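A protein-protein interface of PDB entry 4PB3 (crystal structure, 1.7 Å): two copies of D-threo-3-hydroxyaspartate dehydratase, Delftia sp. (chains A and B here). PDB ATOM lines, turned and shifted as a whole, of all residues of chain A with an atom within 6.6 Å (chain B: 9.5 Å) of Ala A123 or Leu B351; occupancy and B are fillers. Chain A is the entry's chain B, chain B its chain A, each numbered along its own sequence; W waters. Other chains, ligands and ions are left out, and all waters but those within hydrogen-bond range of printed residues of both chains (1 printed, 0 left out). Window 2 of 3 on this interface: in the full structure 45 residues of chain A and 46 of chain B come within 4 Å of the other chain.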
ATOM      1  N   MET A  97       1.060  17.550  17.049  1.00  0.00           N
ATOM      2  CA  MET A  97       1.601  16.511  17.931  1.00  0.00           C
ATOM      3  C   MET A  97       0.898  16.512  19.306  1.00  0.00           C
ATOM      4  O   MET A  97       0.850  17.569  19.970  1.00  0.00           O
ATOM      5  CB  MET A  97       3.118  16.783  18.091  1.00  0.00           C
ATOM      6  CG  MET A  97       3.744  15.679  19.000  1.00  0.00           C
ATOM      7  SD  MET A  97       3.579  14.036  18.230  1.00  0.00           S
ATOM      8  CE  MET A  97       4.451  13.047  19.489  1.00  0.00           C
ATOM      9  N   ALA A  98       0.471  15.347  19.739  1.00  0.00           N
ATOM     10  CA  ALA A  98      -0.091  15.223  21.095  1.00  0.00           C
ATOM     11  C   ALA A  98       1.084  14.873  22.020  1.00  0.00           C
ATOM     12  O   ALA A  98       1.841  13.923  21.776  1.00  0.00           O
ATOM     13  CB  ALA A  98      -1.093  14.032  21.142  1.00  0.00           C
ATOM     14  N   PRO A  99       1.167  15.534  23.163  1.00  0.00           N
ATOM     15  CA  PRO A  99       2.292  15.275  24.075  1.00  0.00           C
ATOM     16  C   PRO A  99       2.350  13.829  24.477  1.00  0.00           C
ATOM     17  O   PRO A  99       3.481  13.285  24.714  1.00  0.00           O
ATOM     18  CB  PRO A  99       1.921  16.178  25.316  1.00  0.00           C
ATOM     19  CG  PRO A  99       1.281  17.423  24.612  1.00  0.00           C
ATOM     20  CD  PRO A  99       0.409  16.804  23.484  1.00  0.00           C
ATOM     21  N   SER A 121       1.135  25.595  18.361  1.00  0.00           N
ATOM     22  CA  SER A 121       0.835  26.297  19.589  1.00  0.00           C
ATOM     23  C   SER A 121       2.096  26.350  20.468  1.00  0.00           C
ATOM     24  O   SER A 121       2.959  25.477  20.423  1.00  0.00           O
ATOM     25  CB  SER A 121      -0.296  25.543  20.412  1.00  0.00           C
ATOM     26  OG  SER A 121       0.093  24.250  20.813  1.00  0.00           O
ATOM     27  N   VAL A 122       2.046  27.363  21.327  1.00  0.00           N
ATOM     28  CA  VAL A 122       3.124  27.517  22.334  1.00  0.00           C
ATOM     29  C   VAL A 122       3.089  26.259  23.254  1.00  0.00           C
ATOM     30  O   VAL A 122       4.158  25.710  23.599  1.00  0.00           O
ATOM     31  CB  VAL A 122       3.027  28.820  23.115  1.00  0.00           C
ATOM     32  CG1 VAL A 122       4.088  28.854  24.236  1.00  0.00           C
ATOM     33  CG2 VAL A 122       3.279  29.999  22.142  1.00  0.00           C
ATOM     34  N   ALA A 123       1.886  25.937  23.767  1.00  0.00           N
ATOM     35  CA  ALA A 123       1.898  24.787  24.730  1.00  0.00           C
ATOM     36  C   ALA A 123       2.437  23.491  24.076  1.00  0.00           C
ATOM     37  O   ALA A 123       3.125  22.744  24.794  1.00  0.00           O
ATOM     38  CB  ALA A 123       0.430  24.503  25.176  1.00  0.00           C
ATOM     39  N   ALA A 124       2.111  23.194  22.811  1.00  0.00           N
ATOM     40  CA  ALA A 124       2.653  21.907  22.221  1.00  0.00           C
ATOM     41  C   ALA A 124       4.173  22.051  22.065  1.00  0.00           C
ATOM     42  O   ALA A 124       4.894  21.078  22.318  1.00  0.00           O
ATOM     43  CB  ALA A 124       1.966  21.594  20.862  1.00  0.00           C
ATOM     44  N   ALA A 125       4.641  23.239  21.679  1.00  0.00           N
ATOM     45  CA  ALA A 125       6.107  23.436  21.537  1.00  0.00           C
ATOM     46  C   ALA A 125       6.777  23.265  22.899  1.00  0.00           C
ATOM     47  O   ALA A 125       7.872  22.710  22.994  1.00  0.00           O
ATOM     48  CB  ALA A 125       6.388  24.846  20.977  1.00  0.00           C
ATOM     49  N   GLN A 126       6.150  23.825  23.969  1.00  0.00           N
ATOM     50  CA  GLN A 126       6.716  23.686  25.344  1.00  0.00           C
ATOM     51  C   GLN A 126       6.798  22.196  25.679  1.00  0.00           C
ATOM     52  O   GLN A 126       7.820  21.779  26.343  1.00  0.00           O
ATOM     53  CB  GLN A 126       5.873  24.408  26.401  1.00  0.00           C
ATOM     54  CG  GLN A 126       6.035  25.920  26.250  1.00  0.00           C
ATOM     55  CD  GLN A 126       5.270  26.699  27.305  1.00  0.00           C
ATOM     56  OE1 GLN A 126       4.416  26.052  27.963  1.00  0.00           O
ATOM     57  NE2 GLN A 126       5.496  28.026  27.469  1.00  0.00           N
ATOM     58  N   ALA A 127       5.743  21.419  25.357  1.00  0.00           N
ATOM     59  CA  ALA A 127       5.742  19.995  25.779  1.00  0.00           C
ATOM     60  C   ALA A 127       6.894  19.256  25.071  1.00  0.00           C
ATOM     61  O   ALA A 127       7.600  18.433  25.720  1.00  0.00           O
ATOM     62  CB  ALA A 127       4.427  19.373  25.404  1.00  0.00           C
ATOM     63  N   ILE A 128       7.027  19.498  23.757  1.00  0.00           N
ATOM     64  CA  ILE A 128       8.088  18.791  23.029  1.00  0.00           C
ATOM     65  C   ILE A 128       9.455  19.210  23.586  1.00  0.00           C
ATOM     66  O   ILE A 128      10.330  18.346  23.867  1.00  0.00           O
ATOM     67  CB  ILE A 128       8.008  19.141  21.540  1.00  0.00           C
ATOM     68  CG1 ILE A 128       6.693  18.495  20.955  1.00  0.00           C
ATOM     69  CG2 ILE A 128       9.211  18.439  20.815  1.00  0.00           C
ATOM     70  CD1 ILE A 128       6.572  18.787  19.410  1.00  0.00           C
ATOM     71  N   ILE A 165       6.230  30.551  19.146  1.00  0.00           N
ATOM     72  CA  ILE A 165       6.400  29.127  18.970  1.00  0.00           C
ATOM     73  C   ILE A 165       7.806  28.787  18.500  1.00  0.00           C
ATOM     74  O   ILE A 165       8.458  27.876  19.029  1.00  0.00           O
ATOM     75  CB  ILE A 165       5.384  28.608  17.886  1.00  0.00           C
ATOM     76  CG1 ILE A 165       3.989  28.782  18.517  1.00  0.00           C
ATOM     77  CG2 ILE A 165       5.635  27.107  17.600  1.00  0.00           C
ATOM     78  CD1 ILE A 165       2.890  28.631  17.438  1.00  0.00           C
ATOM     79  N   THR A 168      10.192  29.204  21.322  1.00  0.00           N
ATOM     80  CA  THR A 168      10.034  28.126  22.272  1.00  0.00           C
ATOM     81  C   THR A 168      10.848  26.875  21.824  1.00  0.00           C
ATOM     82  O   THR A 168      11.607  26.261  22.661  1.00  0.00           O
ATOM     83  CB  THR A 168       8.544  27.781  22.475  1.00  0.00           C
ATOM     84  OG1 THR A 168       7.928  28.962  23.050  1.00  0.00           O
ATOM     85  CG2 THR A 168       8.382  26.585  23.512  1.00  0.00           C
ATOM     86  N   ALA B 272     -10.870  10.413  22.599  1.00  0.00           N
ATOM     87  CA  ALA B 272     -10.094  11.287  21.730  1.00  0.00           C
ATOM     88  C   ALA B 272      -9.283  12.265  22.575  1.00  0.00           C
ATOM     89  O   ALA B 272      -9.711  12.619  23.715  1.00  0.00           O
ATOM     90  CB  ALA B 272     -11.061  12.081  20.823  1.00  0.00           C
ATOM     91  N   THR B 273      -8.152  12.765  22.046  1.00  0.00           N
ATOM     92  CA  THR B 273      -7.382  13.786  22.791  1.00  0.00           C
ATOM     93  C   THR B 273      -7.480  15.100  22.030  1.00  0.00           C
ATOM     94  O   THR B 273      -7.444  15.138  20.760  1.00  0.00           O
ATOM     95  CB  THR B 273      -5.881  13.342  22.772  1.00  0.00           C
ATOM     96  OG1 THR B 273      -5.774  12.118  23.555  1.00  0.00           O
ATOM     97  CG2 THR B 273      -5.013  14.400  23.391  1.00  0.00           C
ATOM     98  N   VAL B 274      -7.594  16.187  22.808  1.00  0.00           N
ATOM     99  CA  VAL B 274      -7.502  17.545  22.234  1.00  0.00           C
ATOM    100  C   VAL B 274      -6.016  17.830  21.856  1.00  0.00           C
ATOM    101  O   VAL B 274      -5.116  17.792  22.695  1.00  0.00           O
ATOM    102  CB  VAL B 274      -7.969  18.563  23.267  1.00  0.00           C
ATOM    103  CG1 VAL B 274      -7.725  19.981  22.698  1.00  0.00           C
ATOM    104  CG2 VAL B 274      -9.493  18.319  23.472  1.00  0.00           C
ATOM    105  N   ILE B 275      -5.815  18.032  20.543  1.00  0.00           N
ATOM    106  CA  ILE B 275      -4.426  18.324  20.008  1.00  0.00           C
ATOM    107  C   ILE B 275      -4.237  19.739  19.523  1.00  0.00           C
ATOM    108  O   ILE B 275      -3.123  20.087  19.109  1.00  0.00           O
ATOM    109  CB  ILE B 275      -4.135  17.306  18.865  1.00  0.00           C
ATOM    110  CG1 ILE B 275      -5.113  17.537  17.657  1.00  0.00           C
ATOM    111  CG2 ILE B 275      -4.156  15.825  19.375  1.00  0.00           C
ATOM    112  CD1 ILE B 275      -4.749  16.592  16.493  1.00  0.00           C
ATOM    113  N   GLY B 276      -5.210  20.617  19.724  1.00  0.00           N
ATOM    114  CA  GLY B 276      -4.979  22.048  19.399  1.00  0.00           C
ATOM    115  C   GLY B 276      -6.337  22.751  19.363  1.00  0.00           C
ATOM    116  O   GLY B 276      -7.340  22.190  19.798  1.00  0.00           O
ATOM    117  N   HIS B 277      -6.280  23.990  18.897  1.00  0.00           N
ATOM    118  CA  HIS B 277      -7.512  24.843  18.893  1.00  0.00           C
ATOM    119  C   HIS B 277      -7.461  25.773  17.725  1.00  0.00           C
ATOM    120  O   HIS B 277      -6.389  25.965  17.101  1.00  0.00           O
ATOM    121  CB  HIS B 277      -7.571  25.767  20.148  1.00  0.00           C
ATOM    122  CG  HIS B 277      -7.483  24.972  21.368  1.00  0.00           C
ATOM    123  ND1 HIS B 277      -6.276  24.699  21.951  1.00  0.00           N
ATOM    124  CD2 HIS B 277      -8.482  24.310  22.105  1.00  0.00           C
ATOM    125  CE1 HIS B 277      -6.538  23.872  23.104  1.00  0.00           C
ATOM    126  NE2 HIS B 277      -7.846  23.613  23.141  1.00  0.00           N
ATOM    127  N   ALA B 284     -12.037  23.336  19.180  1.00  0.00           N
ATOM    128  CA  ALA B 284     -10.949  22.483  19.761  1.00  0.00           C
ATOM    129  C   ALA B 284     -10.729  21.402  18.715  1.00  0.00           C
ATOM    130  O   ALA B 284     -11.676  20.827  18.119  1.00  0.00           O
ATOM    131  CB  ALA B 284     -11.415  21.815  21.092  1.00  0.00           C
ATOM    132  N   ILE B 285      -9.458  21.118  18.397  1.00  0.00           N
ATOM    133  CA  ILE B 285      -9.212  20.047  17.418  1.00  0.00           C
ATOM    134  C   ILE B 285      -8.867  18.787  18.192  1.00  0.00           C
ATOM    135  O   ILE B 285      -8.053  18.800  19.122  1.00  0.00           O
ATOM    136  CB  ILE B 285      -7.964  20.426  16.588  1.00  0.00           C
ATOM    137  CG1 ILE B 285      -8.077  21.816  15.987  1.00  0.00           C
ATOM    138  CG2 ILE B 285      -7.729  19.339  15.497  1.00  0.00           C
ATOM    139  CD1 ILE B 285      -9.285  21.988  15.137  1.00  0.00           C
ATOM    140  N   VAL B 286      -9.479  17.689  17.796  1.00  0.00           N
ATOM    141  CA  VAL B 286      -9.269  16.397  18.469  1.00  0.00           C
ATOM    142  C   VAL B 286      -8.690  15.413  17.474  1.00  0.00           C
ATOM    143  O   VAL B 286      -8.783  15.611  16.237  1.00  0.00           O
ATOM    144  CB  VAL B 286     -10.544  15.818  19.108  1.00  0.00           C
ATOM    145  CG1 VAL B 286     -10.982  16.709  20.332  1.00  0.00           C
ATOM    146  CG2 VAL B 286     -11.694  15.627  18.069  1.00  0.00           C
ATOM    147  N   ASP B 287      -8.075  14.346  18.012  1.00  0.00           N
ATOM    148  CA  ASP B 287      -7.469  13.331  17.097  1.00  0.00           C
ATOM    149  C   ASP B 287      -8.432  12.193  16.698  1.00  0.00           C
ATOM    150  O   ASP B 287      -7.956  11.132  16.189  1.00  0.00           O
ATOM    151  CB  ASP B 287      -6.151  12.859  17.750  1.00  0.00           C
ATOM    152  CG  ASP B 287      -6.415  12.011  19.022  1.00  0.00           C
ATOM    153  OD1 ASP B 287      -7.566  11.869  19.471  1.00  0.00           O
ATOM    154  OD2 ASP B 287      -5.374  11.540  19.556  1.00  0.00           O
ATOM    155  N   ILE B 345     -12.018  28.748  24.191  1.00  0.00           N
ATOM    156  CA  ILE B 345     -12.078  27.316  24.090  1.00  0.00           C
ATOM    157  C   ILE B 345     -10.813  26.630  24.674  1.00  0.00           C
ATOM    158  O   ILE B 345     -10.895  25.497  25.163  1.00  0.00           O
ATOM    159  CB  ILE B 345     -12.348  26.925  22.597  1.00  0.00           C
ATOM    160  CG1 ILE B 345     -12.708  25.465  22.370  1.00  0.00           C
ATOM    161  CG2 ILE B 345     -11.114  27.264  21.774  1.00  0.00           C
ATOM    162  CD1 ILE B 345     -14.132  25.046  22.692  1.00  0.00           C
ATOM    163  N   ALA B 346      -9.660  27.242  24.569  1.00  0.00           N
ATOM    164  CA  ALA B 346      -8.390  26.549  25.014  1.00  0.00           C
ATOM    165  C   ALA B 346      -8.314  26.522  26.575  1.00  0.00           C
ATOM    166  O   ALA B 346      -7.736  25.593  27.190  1.00  0.00           O
ATOM    167  CB  ALA B 346      -7.177  27.246  24.400  1.00  0.00           C
ATOM    168  N   THR B 347      -8.980  27.465  27.196  1.00  0.00           N
ATOM    169  CA  THR B 347      -8.970  27.474  28.694  1.00  0.00           C
ATOM    170  C   THR B 347      -9.999  26.386  29.189  1.00  0.00           C
ATOM    171  O   THR B 347      -9.738  25.727  30.226  1.00  0.00           O
ATOM    172  CB  THR B 347      -9.333  28.823  29.259  1.00  0.00           C
ATOM    173  OG1 THR B 347     -10.692  29.116  28.896  1.00  0.00           O
ATOM    174  CG2 THR B 347      -8.364  29.898  28.867  1.00  0.00           C
ATOM    175  N   ARG B 348     -11.075  26.104  28.442  1.00  0.00           N
ATOM    176  CA  ARG B 348     -11.974  25.000  28.754  1.00  0.00           C
ATOM    177  C   ARG B 348     -11.417  23.617  28.475  1.00  0.00           C
ATOM    178  O   ARG B 348     -11.639  22.629  29.196  1.00  0.00           O
ATOM    179  CB  ARG B 348     -13.322  25.178  28.057  1.00  0.00           C
ATOM    180  CG  ARG B 348     -14.237  23.997  28.286  1.00  0.00           C
ATOM    181  CD  ARG B 348     -15.215  24.106  29.477  1.00  0.00           C
ATOM    182  NE  ARG B 348     -16.216  25.032  28.868  1.00  0.00           N
ATOM    183  CZ  ARG B 348     -17.532  24.815  28.610  1.00  0.00           C
ATOM    184  NH1 ARG B 348     -18.149  23.723  29.015  1.00  0.00           N
ATOM    185  NH2 ARG B 348     -18.238  25.786  27.979  1.00  0.00           N
ATOM    186  N   PHE B 349     -10.722  23.506  27.337  1.00  0.00           N
ATOM    187  CA  PHE B 349     -10.268  22.166  26.885  1.00  0.00           C
ATOM    188  C   PHE B 349      -8.794  22.286  26.586  1.00  0.00           C
ATOM    189  O   PHE B 349      -8.453  22.346  25.372  1.00  0.00           O
ATOM    190  CB  PHE B 349     -10.998  21.795  25.526  1.00  0.00           C
ATOM    191  CG  PHE B 349     -12.491  21.555  25.675  1.00  0.00           C
ATOM    192  CD1 PHE B 349     -12.991  20.469  26.446  1.00  0.00           C
ATOM    193  CD2 PHE B 349     -13.372  22.481  25.076  1.00  0.00           C
ATOM    194  CE1 PHE B 349     -14.420  20.363  26.585  1.00  0.00           C
ATOM    195  CE2 PHE B 349     -14.752  22.357  25.173  1.00  0.00           C
ATOM    196  CZ  PHE B 349     -15.274  21.294  25.901  1.00  0.00           C
ATOM    197  N   PRO B 350      -7.930  22.303  27.617  1.00  0.00           N
ATOM    198  CA  PRO B 350      -6.503  22.522  27.342  1.00  0.00           C
ATOM    199  C   PRO B 350      -5.943  21.350  26.540  1.00  0.00           C
ATOM    200  O   PRO B 350      -6.468  20.216  26.491  1.00  0.00           O
ATOM    201  CB  PRO B 350      -5.817  22.546  28.759  1.00  0.00           C
ATOM    202  CG  PRO B 350      -6.955  22.690  29.804  1.00  0.00           C
ATOM    203  CD  PRO B 350      -8.231  22.274  29.095  1.00  0.00           C
ATOM    204  N   LEU B 351      -4.814  21.667  25.830  1.00  0.00           N
ATOM    205  CA  LEU B 351      -4.096  20.551  25.084  1.00  0.00           C
ATOM    206  C   LEU B 351      -3.953  19.299  25.959  1.00  0.00           C
ATOM    207  O   LEU B 351      -3.509  19.403  27.134  1.00  0.00           O
ATOM    208  CB  LEU B 351      -2.653  21.152  24.772  1.00  0.00           C
ATOM    209  CG  LEU B 351      -1.765  20.177  23.974  1.00  0.00           C
ATOM    210  CD1 LEU B 351      -2.321  19.920  22.559  1.00  0.00           C
ATOM    211  CD2 LEU B 351      -0.364  20.830  23.941  1.00  0.00           C
ATOM    212  N   GLY B 352      -4.257  18.160  25.386  1.00  0.00           N
ATOM    213  CA  GLY B 352      -4.065  16.866  25.995  1.00  0.00           C
ATOM    214  C   GLY B 352      -5.352  16.435  26.754  1.00  0.00           C
ATOM    215  O   GLY B 352      -5.429  15.261  27.169  1.00  0.00           O
ATOM    216  N   THR B 353      -6.354  17.305  26.868  1.00  0.00           N
ATOM    217  CA  THR B 353      -7.669  16.866  27.499  1.00  0.00           C
ATOM    218  C   THR B 353      -8.231  15.711  26.727  1.00  0.00           C
ATOM    219  O   THR B 353      -8.294  15.727  25.479  1.00  0.00           O
ATOM    220  CB  THR B 353      -8.634  18.044  27.495  1.00  0.00           C
ATOM    221  OG1 THR B 353      -8.095  19.115  28.263  1.00  0.00           O
ATOM    222  CG2 THR B 353     -10.066  17.624  28.153  1.00  0.00           C
ATOM    223  N   ARG B 354      -8.786  14.728  27.440  1.00  0.00           N
ATOM    224  CA  ARG B 354      -9.426  13.597  26.765  1.00  0.00           C
ATOM    225  C   ARG B 354     -10.943  13.699  26.877  1.00  0.00           C
ATOM    226  O   ARG B 354     -11.475  14.103  27.942  1.00  0.00           O
ATOM    227  CB  ARG B 354      -8.979  12.281  27.371  1.00  0.00           C
ATOM    228  CG  ARG B 354      -7.502  12.062  27.055  1.00  0.00           C
ATOM    229  CD  ARG B 354      -7.034  10.797  27.694  1.00  0.00           C
ATOM    230  NE  ARG B 354      -5.649  10.591  27.114  1.00  0.00           N
ATOM    231  CZ  ARG B 354      -5.180   9.423  26.669  1.00  0.00           C
ATOM    232  NH1 ARG B 354      -5.798   8.312  26.903  1.00  0.00           N
ATOM    233  NH2 ARG B 354      -3.953   9.430  26.077  1.00  0.00           N
HETATM  234  O   HOH W   1      -0.472  19.986  19.205  1.00  0.00           O
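The backbone NH of Ile B275 sits at hydrogen-bond distance from the backbone carbonyl oxygen of Ile B285 (2.8 Å). The side-chain hydroxyl of Ser A121 sits at hydrogen-bond distance from the backbone NH of Ala A124, 3.0 Å away.
Among the printed residues, merely in contact across the chains: Ala A98 with Ile B275, Pro A99 with Leu B351, Ala A123 with Leu B351 and Ala A124 with Leu B351.
Ala A123 touches one residue of chain B. Printed residues of chain A within 4 Å of Leu B351: Pro A99, Ala A123 and Ala A124. No residue of chain B comes within 4 Å of Val A122. Printed residues of chain B within 4 Å of Ala A124: Leu B351. No residue of chain B comes within 4 Å of Ala A125. Of the printed residues of chain A, Ile B275 touches Ala A98. Of the printed residues of chain B, Ala A98 touches Ile B275 (3.96 Å). Phe B349 touches none of the printed residues of chain A. Ser A121 touches none of the printed residues of chain B. The nearest residue of chain A that does not touch Leu B351 is Ser A121 (4.7 Å). The nearest printed residue of chain A that does not touch Ile B275 is Met A97 (4.8 Å).
Printed residues of chain B that touch a printed residue of chain A: Ile B275 and Leu B351. Along chain B the printed residues that touch a printed residue of chain A span positions 275 to 351. Among the printed residues, 4 pairs touch across the chains.
No position is printed for both chains. Of the 4 pairs that touch across the chains among the printed residues, none has its exchanged pair printed and touching as well.
Water W1 lies within hydrogen-bond range of the backbone carbonyl oxygen of Ile B275 (2.7 Å) and the backbone carbonyl oxygen of Met A97 (2.9 Å).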
